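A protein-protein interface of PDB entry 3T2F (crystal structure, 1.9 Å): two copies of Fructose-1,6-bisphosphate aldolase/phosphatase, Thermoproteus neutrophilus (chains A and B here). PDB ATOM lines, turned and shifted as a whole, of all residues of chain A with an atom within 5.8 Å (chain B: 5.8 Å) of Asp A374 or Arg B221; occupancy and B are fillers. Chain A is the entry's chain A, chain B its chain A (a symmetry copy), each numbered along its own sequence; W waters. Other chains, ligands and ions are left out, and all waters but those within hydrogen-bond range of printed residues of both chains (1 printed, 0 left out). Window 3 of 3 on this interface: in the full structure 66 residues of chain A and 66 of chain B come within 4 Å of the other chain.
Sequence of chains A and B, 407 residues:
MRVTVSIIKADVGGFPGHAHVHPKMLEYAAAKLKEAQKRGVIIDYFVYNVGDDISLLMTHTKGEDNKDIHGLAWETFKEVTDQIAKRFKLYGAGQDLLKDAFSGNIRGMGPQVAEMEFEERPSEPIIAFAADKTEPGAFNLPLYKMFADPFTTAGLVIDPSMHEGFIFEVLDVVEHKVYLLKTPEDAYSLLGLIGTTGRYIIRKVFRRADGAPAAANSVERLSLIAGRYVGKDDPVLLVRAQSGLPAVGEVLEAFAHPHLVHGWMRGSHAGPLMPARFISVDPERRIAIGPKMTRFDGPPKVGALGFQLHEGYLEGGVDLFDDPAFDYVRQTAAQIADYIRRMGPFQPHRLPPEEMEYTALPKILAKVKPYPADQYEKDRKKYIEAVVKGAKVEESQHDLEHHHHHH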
ATOM      1  N   PRO A 372      28.559  10.867  -2.621  1.00  0.00           N
ATOM      2  CA  PRO A 372      27.358  10.037  -2.322  1.00  0.00           C
ATOM      3  C   PRO A 372      26.154  10.951  -2.134  1.00  0.00           C
ATOM      4  O   PRO A 372      26.263  11.959  -1.397  1.00  0.00           O
ATOM      5  CB  PRO A 372      27.722   9.306  -0.993  1.00  0.00           C
ATOM      6  CG  PRO A 372      29.280   9.236  -1.058  1.00  0.00           C
ATOM      7  CD  PRO A 372      29.765  10.474  -1.852  1.00  0.00           C
ATOM      8  N   ALA A 373      25.032  10.635  -2.802  1.00  0.00           N
ATOM      9  CA  ALA A 373      23.853  11.503  -2.801  1.00  0.00           C
ATOM     10  C   ALA A 373      23.258  11.759  -1.412  1.00  0.00           C
ATOM     11  O   ALA A 373      22.759  12.846  -1.158  1.00  0.00           O
ATOM     12  CB  ALA A 373      22.775  11.011  -3.763  1.00  0.00           C
ATOM     13  N   ASP A 374      23.335  10.767  -0.520  1.00  0.00           N
ATOM     14  CA  ASP A 374      22.856  10.903   0.888  1.00  0.00           C
ATOM     15  C   ASP A 374      23.608  11.933   1.714  1.00  0.00           C
ATOM     16  O   ASP A 374      23.048  12.861   2.298  1.00  0.00           O
ATOM     17  CB  ASP A 374      22.904   9.546   1.546  1.00  0.00           C
ATOM     18  CG  ASP A 374      21.720   8.708   1.137  1.00  0.00           C
ATOM     19  OD1 ASP A 374      20.649   9.298   0.902  1.00  0.00           O
ATOM     20  OD2 ASP A 374      21.833   7.476   1.043  1.00  0.00           O
ATOM     21  N   GLN A 375      24.903  11.804   1.715  1.00  0.00           N
ATOM     22  CA  GLN A 375      25.662  12.730   2.454  1.00  0.00           C
ATOM     23  C   GLN A 375      25.619  14.094   1.818  1.00  0.00           C
ATOM     24  O   GLN A 375      25.574  15.104   2.533  1.00  0.00           O
ATOM     25  CB  GLN A 375      27.066  12.212   2.678  1.00  0.00           C
ATOM     26  CG  GLN A 375      28.080  12.344   1.562  1.00  0.00           C
ATOM     27  CD  GLN A 375      29.525  12.166   2.104  1.00  0.00           C
ATOM     28  OE1 GLN A 375      30.437  11.699   1.402  1.00  0.00           O
ATOM     29  NE2 GLN A 375      29.719  12.540   3.375  1.00  0.00           N
ATOM     30  N   TYR A 376      25.592  14.127   0.476  1.00  0.00           N
ATOM     31  CA  TYR A 376      25.546  15.412  -0.252  1.00  0.00           C
ATOM     32  C   TYR A 376      24.428  16.310   0.217  1.00  0.00           C
ATOM     33  O   TYR A 376      24.685  17.469   0.490  1.00  0.00           O
ATOM     34  CB  TYR A 376      25.461  15.257  -1.784  1.00  0.00           C
ATOM     35  CG  TYR A 376      25.374  16.604  -2.491  1.00  0.00           C
ATOM     36  CD1 TYR A 376      24.120  17.183  -2.799  1.00  0.00           C
ATOM     37  CD2 TYR A 376      26.528  17.312  -2.793  1.00  0.00           C
ATOM     38  CE1 TYR A 376      24.069  18.483  -3.479  1.00  0.00           C
ATOM     39  CE2 TYR A 376      26.490  18.574  -3.441  1.00  0.00           C
ATOM     40  CZ  TYR A 376      25.260  19.131  -3.769  1.00  0.00           C
ATOM     41  OH  TYR A 376      25.254  20.349  -4.415  1.00  0.00           O
ATOM     42  N   GLU A 377      23.206  15.792   0.272  1.00  0.00           N
ATOM     43  CA  GLU A 377      22.047  16.542   0.785  1.00  0.00           C
ATOM     44  C   GLU A 377      22.305  17.314   2.085  1.00  0.00           C
ATOM     45  O   GLU A 377      21.987  18.518   2.193  1.00  0.00           O
ATOM     46  CB  GLU A 377      20.926  15.568   1.122  1.00  0.00           C
ATOM     47  CG  GLU A 377      20.330  14.811  -0.042  1.00  0.00           C
ATOM     48  CD  GLU A 377      19.228  15.618  -0.776  1.00  0.00           C
ATOM     49  OE1 GLU A 377      19.048  16.811  -0.450  1.00  0.00           O
ATOM     50  OE2 GLU A 377      18.556  15.046  -1.666  1.00  0.00           O
ATOM     51  N   LYS A 378      22.867  16.613   3.072  1.00  0.00           N
ATOM     52  CA  LYS A 378      23.180  17.226   4.386  1.00  0.00           C
ATOM     53  C   LYS A 378      24.080  18.445   4.265  1.00  0.00           C
ATOM     54  O   LYS A 378      23.878  19.426   4.959  1.00  0.00           O
ATOM     55  CB  LYS A 378      23.837  16.184   5.328  1.00  0.00           C
ATOM     56  CG  LYS A 378      23.179  16.111   6.782  1.00  0.00           C
ATOM     57  CD  LYS A 378      23.595  14.827   7.599  1.00  0.00           C
ATOM     58  CE  LYS A 378      23.069  13.489   7.008  1.00  0.00           C
ATOM     59  NZ  LYS A 378      23.992  12.962   5.931  1.00  0.00           N
ATOM     60  N   LEU B 171      22.715  14.897 -10.730  1.00  0.00           N
ATOM     61  CA  LEU B 171      22.431  13.651 -10.064  1.00  0.00           C
ATOM     62  C   LEU B 171      22.568  12.456 -11.028  1.00  0.00           C
ATOM     63  O   LEU B 171      21.877  12.405 -12.069  1.00  0.00           O
ATOM     64  CB  LEU B 171      21.038  13.666  -9.479  1.00  0.00           C
ATOM     65  CG  LEU B 171      20.539  12.403  -8.740  1.00  0.00           C
ATOM     66  CD1 LEU B 171      21.357  12.139  -7.418  1.00  0.00           C
ATOM     67  CD2 LEU B 171      19.042  12.583  -8.380  1.00  0.00           C
ATOM     68  N   ASP B 172      23.434  11.503 -10.676  1.00  0.00           N
ATOM     69  CA  ASP B 172      23.414  10.176 -11.317  1.00  0.00           C
ATOM     70  C   ASP B 172      22.315   9.419 -10.635  1.00  0.00           C
ATOM     71  O   ASP B 172      22.412   9.008  -9.373  1.00  0.00           O
ATOM     72  CB  ASP B 172      24.810   9.550 -11.051  1.00  0.00           C
ATOM     73  CG  ASP B 172      24.930   8.112 -11.565  1.00  0.00           C
ATOM     74  OD1 ASP B 172      23.906   7.488 -11.865  1.00  0.00           O
ATOM     75  OD2 ASP B 172      26.067   7.589 -11.617  1.00  0.00           O
ATOM     76  N   VAL B 173      21.235   9.194 -11.354  1.00  0.00           N
ATOM     77  CA  VAL B 173      20.120   8.633 -10.656  1.00  0.00           C
ATOM     78  C   VAL B 173      20.237   7.060 -10.548  1.00  0.00           C
ATOM     79  O   VAL B 173      19.411   6.412  -9.869  1.00  0.00           O
ATOM     80  CB  VAL B 173      18.816   8.934 -11.388  1.00  0.00           C
ATOM     81  CG1 VAL B 173      18.599  10.472 -11.447  1.00  0.00           C
ATOM     82  CG2 VAL B 173      18.770   8.275 -12.838  1.00  0.00           C
ATOM     83  N   VAL B 174      21.206   6.494 -11.255  1.00  0.00           N
ATOM     84  CA  VAL B 174      21.397   5.016 -11.211  1.00  0.00           C
ATOM     85  C   VAL B 174      22.297   4.650  -9.980  1.00  0.00           C
ATOM     86  O   VAL B 174      21.873   3.868  -9.138  1.00  0.00           O
ATOM     87  CB  VAL B 174      22.001   4.502 -12.514  1.00  0.00           C
ATOM     88  CG1 VAL B 174      22.377   2.970 -12.400  1.00  0.00           C
ATOM     89  CG2 VAL B 174      20.989   4.785 -13.672  1.00  0.00           C
ATOM     90  N   HIS B 176      23.227   6.816  -7.599  1.00  0.00           N
ATOM     91  CA  HIS B 176      22.970   7.817  -6.522  1.00  0.00           C
ATOM     92  C   HIS B 176      24.245   8.589  -6.106  1.00  0.00           C
ATOM     93  O   HIS B 176      24.659   8.544  -4.927  1.00  0.00           O
ATOM     94  CB  HIS B 176      22.368   7.236  -5.216  1.00  0.00           C
ATOM     95  CG  HIS B 176      21.228   6.257  -5.367  1.00  0.00           C
ATOM     96  ND1 HIS B 176      20.910   5.600  -6.546  1.00  0.00           N
ATOM     97  CD2 HIS B 176      20.367   5.765  -4.430  1.00  0.00           C
ATOM     98  CE1 HIS B 176      19.855   4.817  -6.347  1.00  0.00           C
ATOM     99  NE2 HIS B 176      19.505   4.899  -5.074  1.00  0.00           N
ATOM    100  N   LYS B 177      24.887   9.266  -7.052  1.00  0.00           N
ATOM    101  CA  LYS B 177      26.081  10.095  -6.873  1.00  0.00           C
ATOM    102  C   LYS B 177      25.789  11.478  -7.413  1.00  0.00           C
ATOM    103  O   LYS B 177      25.046  11.595  -8.419  1.00  0.00           O
ATOM    104  CB  LYS B 177      27.248   9.514  -7.639  1.00  0.00           C
ATOM    105  CG  LYS B 177      27.669   8.143  -6.990  1.00  0.00           C
ATOM    106  CD  LYS B 177      28.721   7.467  -7.775  1.00  0.00           C
ATOM    107  CE  LYS B 177      29.228   6.202  -7.041  1.00  0.00           C
ATOM    108  NZ  LYS B 177      29.687   5.265  -8.121  1.00  0.00           N
ATOM    109  N   ARG B 203      19.958  18.718 -11.490  1.00  0.00           N
ATOM    110  CA  ARG B 203      18.907  18.851 -10.463  1.00  0.00           C
ATOM    111  C   ARG B 203      18.828  20.338  -9.952  1.00  0.00           C
ATOM    112  O   ARG B 203      17.727  20.829  -9.677  1.00  0.00           O
ATOM    113  CB  ARG B 203      19.252  17.935  -9.232  1.00  0.00           C
ATOM    114  CG  ARG B 203      18.144  17.962  -8.144  1.00  0.00           C
ATOM    115  CD  ARG B 203      18.372  16.760  -7.158  1.00  0.00           C
ATOM    116  NE  ARG B 203      19.679  16.859  -6.511  1.00  0.00           N
ATOM    117  CZ  ARG B 203      20.142  15.931  -5.642  1.00  0.00           C
ATOM    118  NH1 ARG B 203      19.392  14.868  -5.304  1.00  0.00           N
ATOM    119  NH2 ARG B 203      21.314  16.124  -5.056  1.00  0.00           N
ATOM    120  N   VAL B 219      13.893  15.719  -9.872  1.00  0.00           N
ATOM    121  CA  VAL B 219      14.476  14.435 -10.191  1.00  0.00           C
ATOM    122  C   VAL B 219      14.886  13.695  -8.904  1.00  0.00           C
ATOM    123  O   VAL B 219      15.379  14.334  -8.011  1.00  0.00           O
ATOM    124  CB  VAL B 219      15.657  14.552 -11.116  1.00  0.00           C
ATOM    125  CG1 VAL B 219      16.833  15.503 -10.587  1.00  0.00           C
ATOM    126  CG2 VAL B 219      16.099  13.108 -11.686  1.00  0.00           C
ATOM    127  N   GLU B 220      14.713  12.376  -8.852  1.00  0.00           N
ATOM    128  CA  GLU B 220      15.117  11.581  -7.637  1.00  0.00           C
ATOM    129  C   GLU B 220      15.920  10.376  -8.168  1.00  0.00           C
ATOM    130  O   GLU B 220      15.784   9.978  -9.359  1.00  0.00           O
ATOM    131  CB  GLU B 220      13.867  11.064  -6.895  1.00  0.00           C
ATOM    132  CG  GLU B 220      12.912  12.163  -6.380  1.00  0.00           C
ATOM    133  CD  GLU B 220      13.629  13.205  -5.468  1.00  0.00           C
ATOM    134  OE1 GLU B 220      13.187  14.412  -5.422  1.00  0.00           O
ATOM    135  OE2 GLU B 220      14.676  12.833  -4.837  1.00  0.00           O
ATOM    136  N   ARG B 221      16.773   9.825  -7.313  1.00  0.00           N
ATOM    137  CA  ARG B 221      17.470   8.586  -7.629  1.00  0.00           C
ATOM    138  C   ARG B 221      16.421   7.538  -8.023  1.00  0.00           C
ATOM    139  O   ARG B 221      15.246   7.648  -7.628  1.00  0.00           O
ATOM    140  CB  ARG B 221      18.338   8.134  -6.442  1.00  0.00           C
ATOM    141  CG  ARG B 221      17.524   7.482  -5.271  1.00  0.00           C
ATOM    142  CD  ARG B 221      17.452   8.418  -4.020  1.00  0.00           C
ATOM    143  NE  ARG B 221      18.668   8.289  -3.195  1.00  0.00           N
ATOM    144  CZ  ARG B 221      19.808   8.972  -3.361  1.00  0.00           C
ATOM    145  NH1 ARG B 221      20.846   8.716  -2.555  1.00  0.00           N
ATOM    146  NH2 ARG B 221      19.929   9.882  -4.338  1.00  0.00           N
ATOM    147  N   LEU B 222      16.751   6.578  -8.877  1.00  0.00           N
ATOM    148  CA  LEU B 222      15.737   5.526  -9.146  1.00  0.00           C
ATOM    149  C   LEU B 222      15.568   4.609  -7.905  1.00  0.00           C
ATOM    150  O   LEU B 222      16.539   4.344  -7.172  1.00  0.00           O
ATOM    151  CB  LEU B 222      16.077   4.703 -10.369  1.00  0.00           C
ATOM    152  CG  LEU B 222      16.280   5.450 -11.683  1.00  0.00           C
ATOM    153  CD1 LEU B 222      16.828   4.465 -12.676  1.00  0.00           C
ATOM    154  CD2 LEU B 222      14.987   6.067 -12.196  1.00  0.00           C
ATOM    155  N   SER B 223      14.324   4.231  -7.615  1.00  0.00           N
ATOM    156  CA  SER B 223      14.033   3.166  -6.646  1.00  0.00           C
ATOM    157  C   SER B 223      13.010   2.280  -7.291  1.00  0.00           C
ATOM    158  O   SER B 223      12.500   2.624  -8.356  1.00  0.00           O
ATOM    159  CB  SER B 223      13.566   3.691  -5.271  1.00  0.00           C
ATOM    160  OG  SER B 223      12.506   4.641  -5.364  1.00  0.00           O
ATOM    161  N   VAL B 230      10.574   4.607  -9.832  1.00  0.00           N
ATOM    162  CA  VAL B 230      10.208   5.986  -9.560  1.00  0.00           C
ATOM    163  C   VAL B 230      11.487   6.806  -9.603  1.00  0.00           C
ATOM    164  O   VAL B 230      12.570   6.303  -9.206  1.00  0.00           O
ATOM    165  CB  VAL B 230       9.451   6.167  -8.177  1.00  0.00           C
ATOM    166  CG1 VAL B 230       8.992   4.842  -7.633  1.00  0.00           C
ATOM    167  CG2 VAL B 230      10.242   6.947  -7.135  1.00  0.00           C
ATOM    168  N   GLY B 231      11.350   8.068 -10.029  1.00  0.00           N
ATOM    169  CA  GLY B 231      12.439   9.081  -9.924  1.00  0.00           C
ATOM    170  C   GLY B 231      12.382   9.993 -11.142  1.00  0.00           C
ATOM    171  O   GLY B 231      12.620  11.246 -11.042  1.00  0.00           O
HETATM  172  O   HOH W   1      21.176  14.491  -2.788  1.00  0.00           O
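Pro A372 touches His B176 (C to O, 3.98 Å). Ala A373 touches Arg B221 (CB to NH2, 3.1 Å). Tyr A376 touches Arg B203 (CD1 to NH2, 3.8 Å).
Printed residues of chain B within 4 Å of Pro A372: His B176 (3.98 Å). Printed residues of chain B within 4 Å of Ala A373: His B176 and Arg B221. Gln A375 touches none of the printed residues of chain B. Of the printed residues of chain B, Tyr A376 touches Arg B203. Val B219 touches none of the printed residues of chain A. Arg B221 touches just these residues of chain A: Ala A373 and Asp A374. The nearest printed residue of chain B that does not touch Tyr A376 is Lys B177 (6.8 Å).
Water W1 lies within hydrogen-bond range of the guanidinium group (NH2) of Arg B203 (2.8 Å), the backbone carbonyl oxygen (O) of Ala A373 (2.8 Å) and the side-chain carboxylate (OE2) of Glu A377 (2.9 Å).
The guanidinium group (NH1) of Arg B203 is in salt-bridge range of the side-chain carboxylate (OE2) of Glu A377, at 3.7 Å. The guanidinium group (NH1) of Arg B221 lies within salt-bridge range of the side-chain carboxylate (OD1) of Asp A374 (3.5 Å). The backbone carbonyl oxygen (O) of His B176 sits at hydrogen-bond distance from the backbone NH (N) of Ala A373 (3.0 Å).
Of the 14 printed residues of chain B, 3 touch a printed residue of chain A. Printed residues of chain B that touch a printed residue of chain A: His B176, Arg B203 and Arg B221. Among the printed residues, 6 pairs touch across the chains. Among the printed residues, Asp or Glu carboxylates within 4 Å of a Lys or Arg side-chain nitrogen of the other chain: Asp A374 with Arg B221 and Glu A377 with Arg B203.
The backbone carbonyl oxygen (O) of Val B174 is in hydrogen-bond range of a ring nitrogen (ND1) of His B176.
No position is printed for both chains. Of the 6 pairs that touch across the chains among the printed residues, none has its exchanged pair printed and touching as well.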
